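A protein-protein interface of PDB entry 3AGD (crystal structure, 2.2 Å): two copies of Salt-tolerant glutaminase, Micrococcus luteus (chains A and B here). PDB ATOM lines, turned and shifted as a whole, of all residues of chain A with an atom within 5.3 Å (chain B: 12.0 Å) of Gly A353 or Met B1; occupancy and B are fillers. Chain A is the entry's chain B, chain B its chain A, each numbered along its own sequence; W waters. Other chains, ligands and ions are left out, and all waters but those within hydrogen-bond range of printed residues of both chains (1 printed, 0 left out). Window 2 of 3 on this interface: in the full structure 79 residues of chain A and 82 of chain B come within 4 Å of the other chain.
O of His B3 lies within hydrogen-bond range of NH1 of Arg A431 (3.4 Å).
The backbone NH of Met B1 lies close to the side-chain carboxylate of Asp A435, at 3.2 Å.
O of Arg B2 lies within hydrogen-bond range of NH1 of Arg A431, 2.8 Å away.
NH2 of Arg A431 is in salt-bridge range of OD1 of Asp B7 (2.6 Å).
ND1 of His B3 is in hydrogen-bond range of N of Ile B5 (3.2 Å).
The backbone carbonyl oxygen (O) of Leu A344 sits at hydrogen-bond distance from the side-chain hydroxyl (OG1) of Thr A348 (3.2 Å).
The backbone carbonyl oxygen (O) of Arg A431 sits close to the side-chain carboxylate (OD2) of Asp A435.
The guanidinium group of Arg B2 lies within salt-bridge range of the side-chain carboxylate of Asp B7 (2.9 Å).
His B3 touches Leu A344 (NE2 to CB, 3.3 Å).
Leu A344 touches Pro B4.
Leu A347 touches Met B1.
OG1 of Thr A348 touches CE of Met B1, 3.7 Å away.
OG1 of Thr A348 touches CA of His B3, at 3.8 Å.
Met B1 touches Gly A353.
Met B1 touches Arg A431 (CB to O, 3.8 Å).
NH1 of Arg A431 touches CA of Pro B4, 3.4 Å away.
Met B1 touches Leu A432.
Gly A353 touches one residue of chain B.
Of the printed residues of chain B, Thr A348 touches Met B1 and His B3.
No residue of chain B comes within 4 Å of Arg A351.
Gly A428 touches none of the printed residues of chain B.
Arg A431 touches just these residues of chain B: Met B1 (3.8 Å), Arg B2 (2.8 Å), His B3 (3.4 Å), Pro B4 (3.4 Å) and Asp B7 (2.6 Å).
Asp A435 touches just one residue of chain B: Met B1.
Printed residues of chain A within 4 Å of Pro B4: Leu A344 and Arg A431.
Of the printed residues of chain A, Asp B7 touches Arg A431.
The nearest printed residue of chain A that does not touch Met B1 is Gly A428 (4.03 Å).
The nearest printed residue of chain B that does not touch Leu A347 is Pro B4 (7.2 Å).
Of the 10 printed residues of chain B, 5 touch a printed residue of chain A.
Hydrophobic or aromatic side chains of chain B that line the printed part of chain A: Met B1, His B3 and Pro B4.
Of the 10 printed residues of chain A, 7 touch a printed residue of chain B.
Along chain A the printed residues that touch a printed residue of chain B span positions 344 to 435.
Among the printed residues, 13 pairs touch across the chains.
Among the printed residues, Asp or Glu carboxylates within 4 Å of a Lys or Arg side-chain nitrogen of the other chain: Arg A431 with Asp B7.
No position is printed for both chains.
Water W1 lies within hydrogen-bond range of N of Gly A353 and N of Met B1.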
ATOM      1  N   LEU A 344     -19.855  22.978   3.820  1.00  0.00           N
ATOM      2  CA  LEU A 344     -20.868  23.366   2.845  1.00  0.00           C
ATOM      3  C   LEU A 344     -21.508  22.130   2.220  1.00  0.00           C
ATOM      4  O   LEU A 344     -22.710  22.111   1.958  1.00  0.00           O
ATOM      5  CB  LEU A 344     -20.249  24.252   1.759  1.00  0.00           C
ATOM      6  CG  LEU A 344     -19.853  25.651   2.236  1.00  0.00           C
ATOM      7  CD1 LEU A 344     -19.068  26.382   1.154  1.00  0.00           C
ATOM      8  CD2 LEU A 344     -21.114  26.428   2.610  1.00  0.00           C
ATOM      9  N   LEU A 347     -24.135  20.887   4.623  1.00  0.00           N
ATOM     10  CA  LEU A 347     -25.317  21.741   4.579  1.00  0.00           C
ATOM     11  C   LEU A 347     -26.142  21.429   3.339  1.00  0.00           C
ATOM     12  O   LEU A 347     -27.351  21.218   3.422  1.00  0.00           O
ATOM     13  CB  LEU A 347     -24.914  23.211   4.549  1.00  0.00           C
ATOM     14  CG  LEU A 347     -24.213  23.747   5.792  1.00  0.00           C
ATOM     15  CD1 LEU A 347     -23.860  25.208   5.581  1.00  0.00           C
ATOM     16  CD2 LEU A 347     -25.122  23.583   6.990  1.00  0.00           C
ATOM     17  N   THR A 348     -25.477  21.403   2.189  1.00  0.00           N
ATOM     18  CA  THR A 348     -26.139  21.118   0.923  1.00  0.00           C
ATOM     19  C   THR A 348     -26.759  19.720   0.896  1.00  0.00           C
ATOM     20  O   THR A 348     -27.790  19.509   0.260  1.00  0.00           O
ATOM     21  CB  THR A 348     -25.148  21.262  -0.255  1.00  0.00           C
ATOM     22  OG1 THR A 348     -24.783  22.640  -0.399  1.00  0.00           O
ATOM     23  CG2 THR A 348     -25.773  20.768  -1.555  1.00  0.00           C
ATOM     24  N   ARG A 351     -30.672  18.718   1.802  1.00  0.00           N
ATOM     25  CA  ARG A 351     -31.801  18.814   0.877  1.00  0.00           C
ATOM     26  C   ARG A 351     -32.922  19.717   1.393  1.00  0.00           C
ATOM     27  O   ARG A 351     -34.100  19.367   1.297  1.00  0.00           O
ATOM     28  CB  ARG A 351     -32.396  17.432   0.590  1.00  0.00           C
ATOM     29  CG  ARG A 351     -31.470  16.426  -0.067  1.00  0.00           C
ATOM     30  CD  ARG A 351     -32.285  15.452  -0.915  1.00  0.00           C
ATOM     31  NE  ARG A 351     -33.603  15.187  -0.336  1.00  0.00           N
ATOM     32  CZ  ARG A 351     -34.574  14.518  -0.955  1.00  0.00           C
ATOM     33  NH1 ARG A 351     -35.740  14.327  -0.352  1.00  0.00           N
ATOM     34  NH2 ARG A 351     -34.380  14.041  -2.176  1.00  0.00           N
ATOM     35  N   THR A 352     -32.564  20.874   1.937  1.00  0.00           N
ATOM     36  CA  THR A 352     -33.568  21.793   2.454  1.00  0.00           C
ATOM     37  C   THR A 352     -34.136  22.674   1.344  1.00  0.00           C
ATOM     38  O   THR A 352     -35.003  23.511   1.592  1.00  0.00           O
ATOM     39  CB  THR A 352     -32.985  22.698   3.553  1.00  0.00           C
ATOM     40  OG1 THR A 352     -31.948  23.518   3.001  1.00  0.00           O
ATOM     41  CG2 THR A 352     -32.412  21.855   4.681  1.00  0.00           C
ATOM     42  N   GLY A 353     -33.646  22.475   0.123  1.00  0.00           N
ATOM     43  CA  GLY A 353     -34.112  23.269  -1.003  1.00  0.00           C
ATOM     44  C   GLY A 353     -35.361  22.723  -1.670  1.00  0.00           C
ATOM     45  O   GLY A 353     -35.487  21.519  -1.887  1.00  0.00           O
ATOM     46  N   GLY A 428     -22.843  29.987   3.634  1.00  0.00           N
ATOM     47  CA  GLY A 428     -23.585  28.749   3.767  1.00  0.00           C
ATOM     48  C   GLY A 428     -24.820  28.969   4.621  1.00  0.00           C
ATOM     49  O   GLY A 428     -25.903  28.464   4.317  1.00  0.00           O
ATOM     50  N   ARG A 431     -27.669  30.938   2.739  1.00  0.00           N
ATOM     51  CA  ARG A 431     -28.431  30.129   1.803  1.00  0.00           C
ATOM     52  C   ARG A 431     -29.358  29.150   2.506  1.00  0.00           C
ATOM     53  O   ARG A 431     -30.381  28.748   1.947  1.00  0.00           O
ATOM     54  CB  ARG A 431     -27.483  29.381   0.861  1.00  0.00           C
ATOM     55  CG  ARG A 431     -26.585  30.321   0.078  1.00  0.00           C
ATOM     56  CD  ARG A 431     -25.889  29.637  -1.074  1.00  0.00           C
ATOM     57  NE  ARG A 431     -25.138  30.610  -1.860  1.00  0.00           N
ATOM     58  CZ  ARG A 431     -24.660  30.381  -3.077  1.00  0.00           C
ATOM     59  NH1 ARG A 431     -24.851  29.204  -3.652  1.00  0.00           N
ATOM     60  NH2 ARG A 431     -24.012  31.340  -3.724  1.00  0.00           N
ATOM     61  N   LEU A 432     -29.002  28.758   3.725  1.00  0.00           N
ATOM     62  CA  LEU A 432     -29.844  27.843   4.480  1.00  0.00           C
ATOM     63  C   LEU A 432     -31.114  28.589   4.846  1.00  0.00           C
ATOM     64  O   LEU A 432     -32.222  28.081   4.684  1.00  0.00           O
ATOM     65  CB  LEU A 432     -29.139  27.372   5.752  1.00  0.00           C
ATOM     66  CG  LEU A 432     -28.510  25.981   5.668  1.00  0.00           C
ATOM     67  CD1 LEU A 432     -27.883  25.624   7.004  1.00  0.00           C
ATOM     68  CD2 LEU A 432     -29.578  24.963   5.292  1.00  0.00           C
ATOM     69  N   ASP A 435     -33.621  29.230   2.378  1.00  0.00           N
ATOM     70  CA  ASP A 435     -34.398  28.036   2.072  1.00  0.00           C
ATOM     71  C   ASP A 435     -35.583  27.942   3.023  1.00  0.00           C
ATOM     72  O   ASP A 435     -36.427  27.055   2.895  1.00  0.00           O
ATOM     73  CB  ASP A 435     -33.536  26.781   2.212  1.00  0.00           C
ATOM     74  CG  ASP A 435     -32.747  26.475   0.960  1.00  0.00           C
ATOM     75  OD1 ASP A 435     -33.358  26.063  -0.047  1.00  0.00           O
ATOM     76  OD2 ASP A 435     -31.515  26.650   0.982  1.00  0.00           O
ATOM     77  N   MET B   1     -30.642  24.145  -0.868  1.00  0.00           N
ATOM     78  CA  MET B   1     -29.738  25.282  -1.208  1.00  0.00           C
ATOM     79  C   MET B   1     -28.697  24.839  -2.227  1.00  0.00           C
ATOM     80  O   MET B   1     -28.499  23.642  -2.450  1.00  0.00           O
ATOM     81  CB  MET B   1     -29.010  25.775   0.040  1.00  0.00           C
ATOM     82  CG  MET B   1     -28.082  24.733   0.647  1.00  0.00           C
ATOM     83  SD  MET B   1     -27.091  25.385   1.996  1.00  0.00           S
ATOM     84  CE  MET B   1     -25.638  25.950   1.107  1.00  0.00           C
ATOM     85  N   ARG B   2     -28.032  25.813  -2.841  1.00  0.00           N
ATOM     86  CA  ARG B   2     -26.994  25.525  -3.820  1.00  0.00           C
ATOM     87  C   ARG B   2     -25.621  25.794  -3.212  1.00  0.00           C
ATOM     88  O   ARG B   2     -25.429  26.775  -2.492  1.00  0.00           O
ATOM     89  CB  ARG B   2     -27.172  26.385  -5.069  1.00  0.00           C
ATOM     90  CG  ARG B   2     -28.493  26.187  -5.783  1.00  0.00           C
ATOM     91  CD  ARG B   2     -28.345  26.518  -7.253  1.00  0.00           C
ATOM     92  NE  ARG B   2     -27.713  27.819  -7.457  1.00  0.00           N
ATOM     93  CZ  ARG B   2     -27.271  28.255  -8.632  1.00  0.00           C
ATOM     94  NH1 ARG B   2     -27.392  27.492  -9.712  1.00  0.00           N
ATOM     95  NH2 ARG B   2     -26.707  29.452  -8.728  1.00  0.00           N
ATOM     96  N   HIS B   3     -24.671  24.914  -3.506  1.00  0.00           N
ATOM     97  CA  HIS B   3     -23.315  25.055  -2.992  1.00  0.00           C
ATOM     98  C   HIS B   3     -22.733  26.364  -3.513  1.00  0.00           C
ATOM     99  O   HIS B   3     -22.801  26.648  -4.704  1.00  0.00           O
ATOM    100  CB  HIS B   3     -22.467  23.875  -3.457  1.00  0.00           C
ATOM    101  CG  HIS B   3     -21.277  23.610  -2.593  1.00  0.00           C
ATOM    102  ND1 HIS B   3     -20.241  24.507  -2.458  1.00  0.00           N
ATOM    103  CD2 HIS B   3     -20.971  22.555  -1.802  1.00  0.00           C
ATOM    104  CE1 HIS B   3     -19.346  24.016  -1.618  1.00  0.00           C
ATOM    105  NE2 HIS B   3     -19.766  22.832  -1.206  1.00  0.00           N
ATOM    106  N   PRO B   4     -22.159  27.186  -2.626  1.00  0.00           N
ATOM    107  CA  PRO B   4     -21.586  28.459  -3.075  1.00  0.00           C
ATOM    108  C   PRO B   4     -20.336  28.388  -3.964  1.00  0.00           C
ATOM    109  O   PRO B   4     -20.110  29.282  -4.781  1.00  0.00           O
ATOM    110  CB  PRO B   4     -21.329  29.207  -1.763  1.00  0.00           C
ATOM    111  CG  PRO B   4     -21.076  28.115  -0.793  1.00  0.00           C
ATOM    112  CD  PRO B   4     -22.117  27.080  -1.158  1.00  0.00           C
ATOM    113  N   ILE B   5     -19.534  27.338  -3.821  1.00  0.00           N
ATOM    114  CA  ILE B   5     -18.317  27.227  -4.623  1.00  0.00           C
ATOM    115  C   ILE B   5     -18.561  27.261  -6.134  1.00  0.00           C
ATOM    116  O   ILE B   5     -17.810  27.899  -6.867  1.00  0.00           O
ATOM    117  CB  ILE B   5     -17.498  25.974  -4.227  1.00  0.00           C
ATOM    118  CG1 ILE B   5     -16.937  26.175  -2.815  1.00  0.00           C
ATOM    119  CG2 ILE B   5     -16.338  25.757  -5.208  1.00  0.00           C
ATOM    120  CD1 ILE B   5     -16.101  25.034  -2.310  1.00  0.00           C
ATOM    121  N   PRO B   6     -19.610  26.574  -6.620  1.00  0.00           N
ATOM    122  CA  PRO B   6     -19.877  26.597  -8.063  1.00  0.00           C
ATOM    123  C   PRO B   6     -20.248  28.013  -8.512  1.00  0.00           C
ATOM    124  O   PRO B   6     -19.952  28.417  -9.637  1.00  0.00           O
ATOM    125  CB  PRO B   6     -21.043  25.623  -8.211  1.00  0.00           C
ATOM    126  CG  PRO B   6     -20.779  24.632  -7.128  1.00  0.00           C
ATOM    127  CD  PRO B   6     -20.409  25.526  -5.963  1.00  0.00           C
ATOM    128  N   ASP B   7     -20.903  28.757  -7.622  1.00  0.00           N
ATOM    129  CA  ASP B   7     -21.301  30.133  -7.909  1.00  0.00           C
ATOM    130  C   ASP B   7     -20.054  31.006  -7.971  1.00  0.00           C
ATOM    131  O   ASP B   7     -19.950  31.909  -8.804  1.00  0.00           O
ATOM    132  CB  ASP B   7     -22.255  30.644  -6.829  1.00  0.00           C
ATOM    133  CG  ASP B   7     -23.653  30.057  -6.958  1.00  0.00           C
ATOM    134  OD1 ASP B   7     -24.476  30.272  -6.043  1.00  0.00           O
ATOM    135  OD2 ASP B   7     -23.931  29.388  -7.977  1.00  0.00           O
ATOM    136  N   TYR B   8     -19.108  30.731  -7.078  1.00  0.00           N
ATOM    137  CA  TYR B   8     -17.853  31.465  -7.059  1.00  0.00           C
ATOM    138  C   TYR B   8     -17.162  31.274  -8.407  1.00  0.00           C
ATOM    139  O   TYR B   8     -16.699  32.230  -9.028  1.00  0.00           O
ATOM    140  CB  TYR B   8     -16.933  30.934  -5.960  1.00  0.00           C
ATOM    141  CG  TYR B   8     -15.498  31.361  -6.163  1.00  0.00           C
ATOM    142  CD1 TYR B   8     -15.066  32.629  -5.779  1.00  0.00           C
ATOM    143  CD2 TYR B   8     -14.594  30.527  -6.819  1.00  0.00           C
ATOM    144  CE1 TYR B   8     -13.771  33.058  -6.051  1.00  0.00           C
ATOM    145  CE2 TYR B   8     -13.297  30.946  -7.097  1.00  0.00           C
ATOM    146  CZ  TYR B   8     -12.895  32.213  -6.714  1.00  0.00           C
ATOM    147  OH  TYR B   8     -11.627  32.644  -7.023  1.00  0.00           O
ATOM    148  N   ARG B  49     -16.720  15.613  -4.458  1.00  0.00           N
ATOM    149  CA  ARG B  49     -17.534  16.630  -5.100  1.00  0.00           C
ATOM    150  C   ARG B  49     -16.816  17.194  -6.312  1.00  0.00           C
ATOM    151  O   ARG B  49     -15.586  17.178  -6.389  1.00  0.00           O
ATOM    152  CB  ARG B  49     -17.852  17.761  -4.116  1.00  0.00           C
ATOM    153  CG  ARG B  49     -18.579  17.296  -2.867  1.00  0.00           C
ATOM    154  CD  ARG B  49     -19.812  16.469  -3.217  1.00  0.00           C
ATOM    155  NE  ARG B  49     -20.379  15.822  -2.037  1.00  0.00           N
ATOM    156  CZ  ARG B  49     -21.154  16.430  -1.144  1.00  0.00           C
ATOM    157  NH1 ARG B  49     -21.472  17.710  -1.294  1.00  0.00           N
ATOM    158  NH2 ARG B  49     -21.595  15.757  -0.089  1.00  0.00           N
ATOM    159  N   HIS B  51     -17.167  20.689  -8.305  1.00  0.00           N
ATOM    160  CA  HIS B  51     -17.742  22.014  -8.489  1.00  0.00           C
ATOM    161  C   HIS B  51     -17.177  22.598  -9.779  1.00  0.00           C
ATOM    162  O   HIS B  51     -15.960  22.683  -9.938  1.00  0.00           O
ATOM    163  CB  HIS B  51     -17.374  22.921  -7.306  1.00  0.00           C
ATOM    164  CG  HIS B  51     -17.625  22.302  -5.964  1.00  0.00           C
ATOM    165  ND1 HIS B  51     -18.853  21.797  -5.593  1.00  0.00           N
ATOM    166  CD2 HIS B  51     -16.806  22.115  -4.901  1.00  0.00           C
ATOM    167  CE1 HIS B  51     -18.779  21.325  -4.360  1.00  0.00           C
ATOM    168  NE2 HIS B  51     -17.549  21.506  -3.917  1.00  0.00           N
HETATM  169  O   HOH W   1     -32.003  21.435  -1.990  1.00  0.00           O
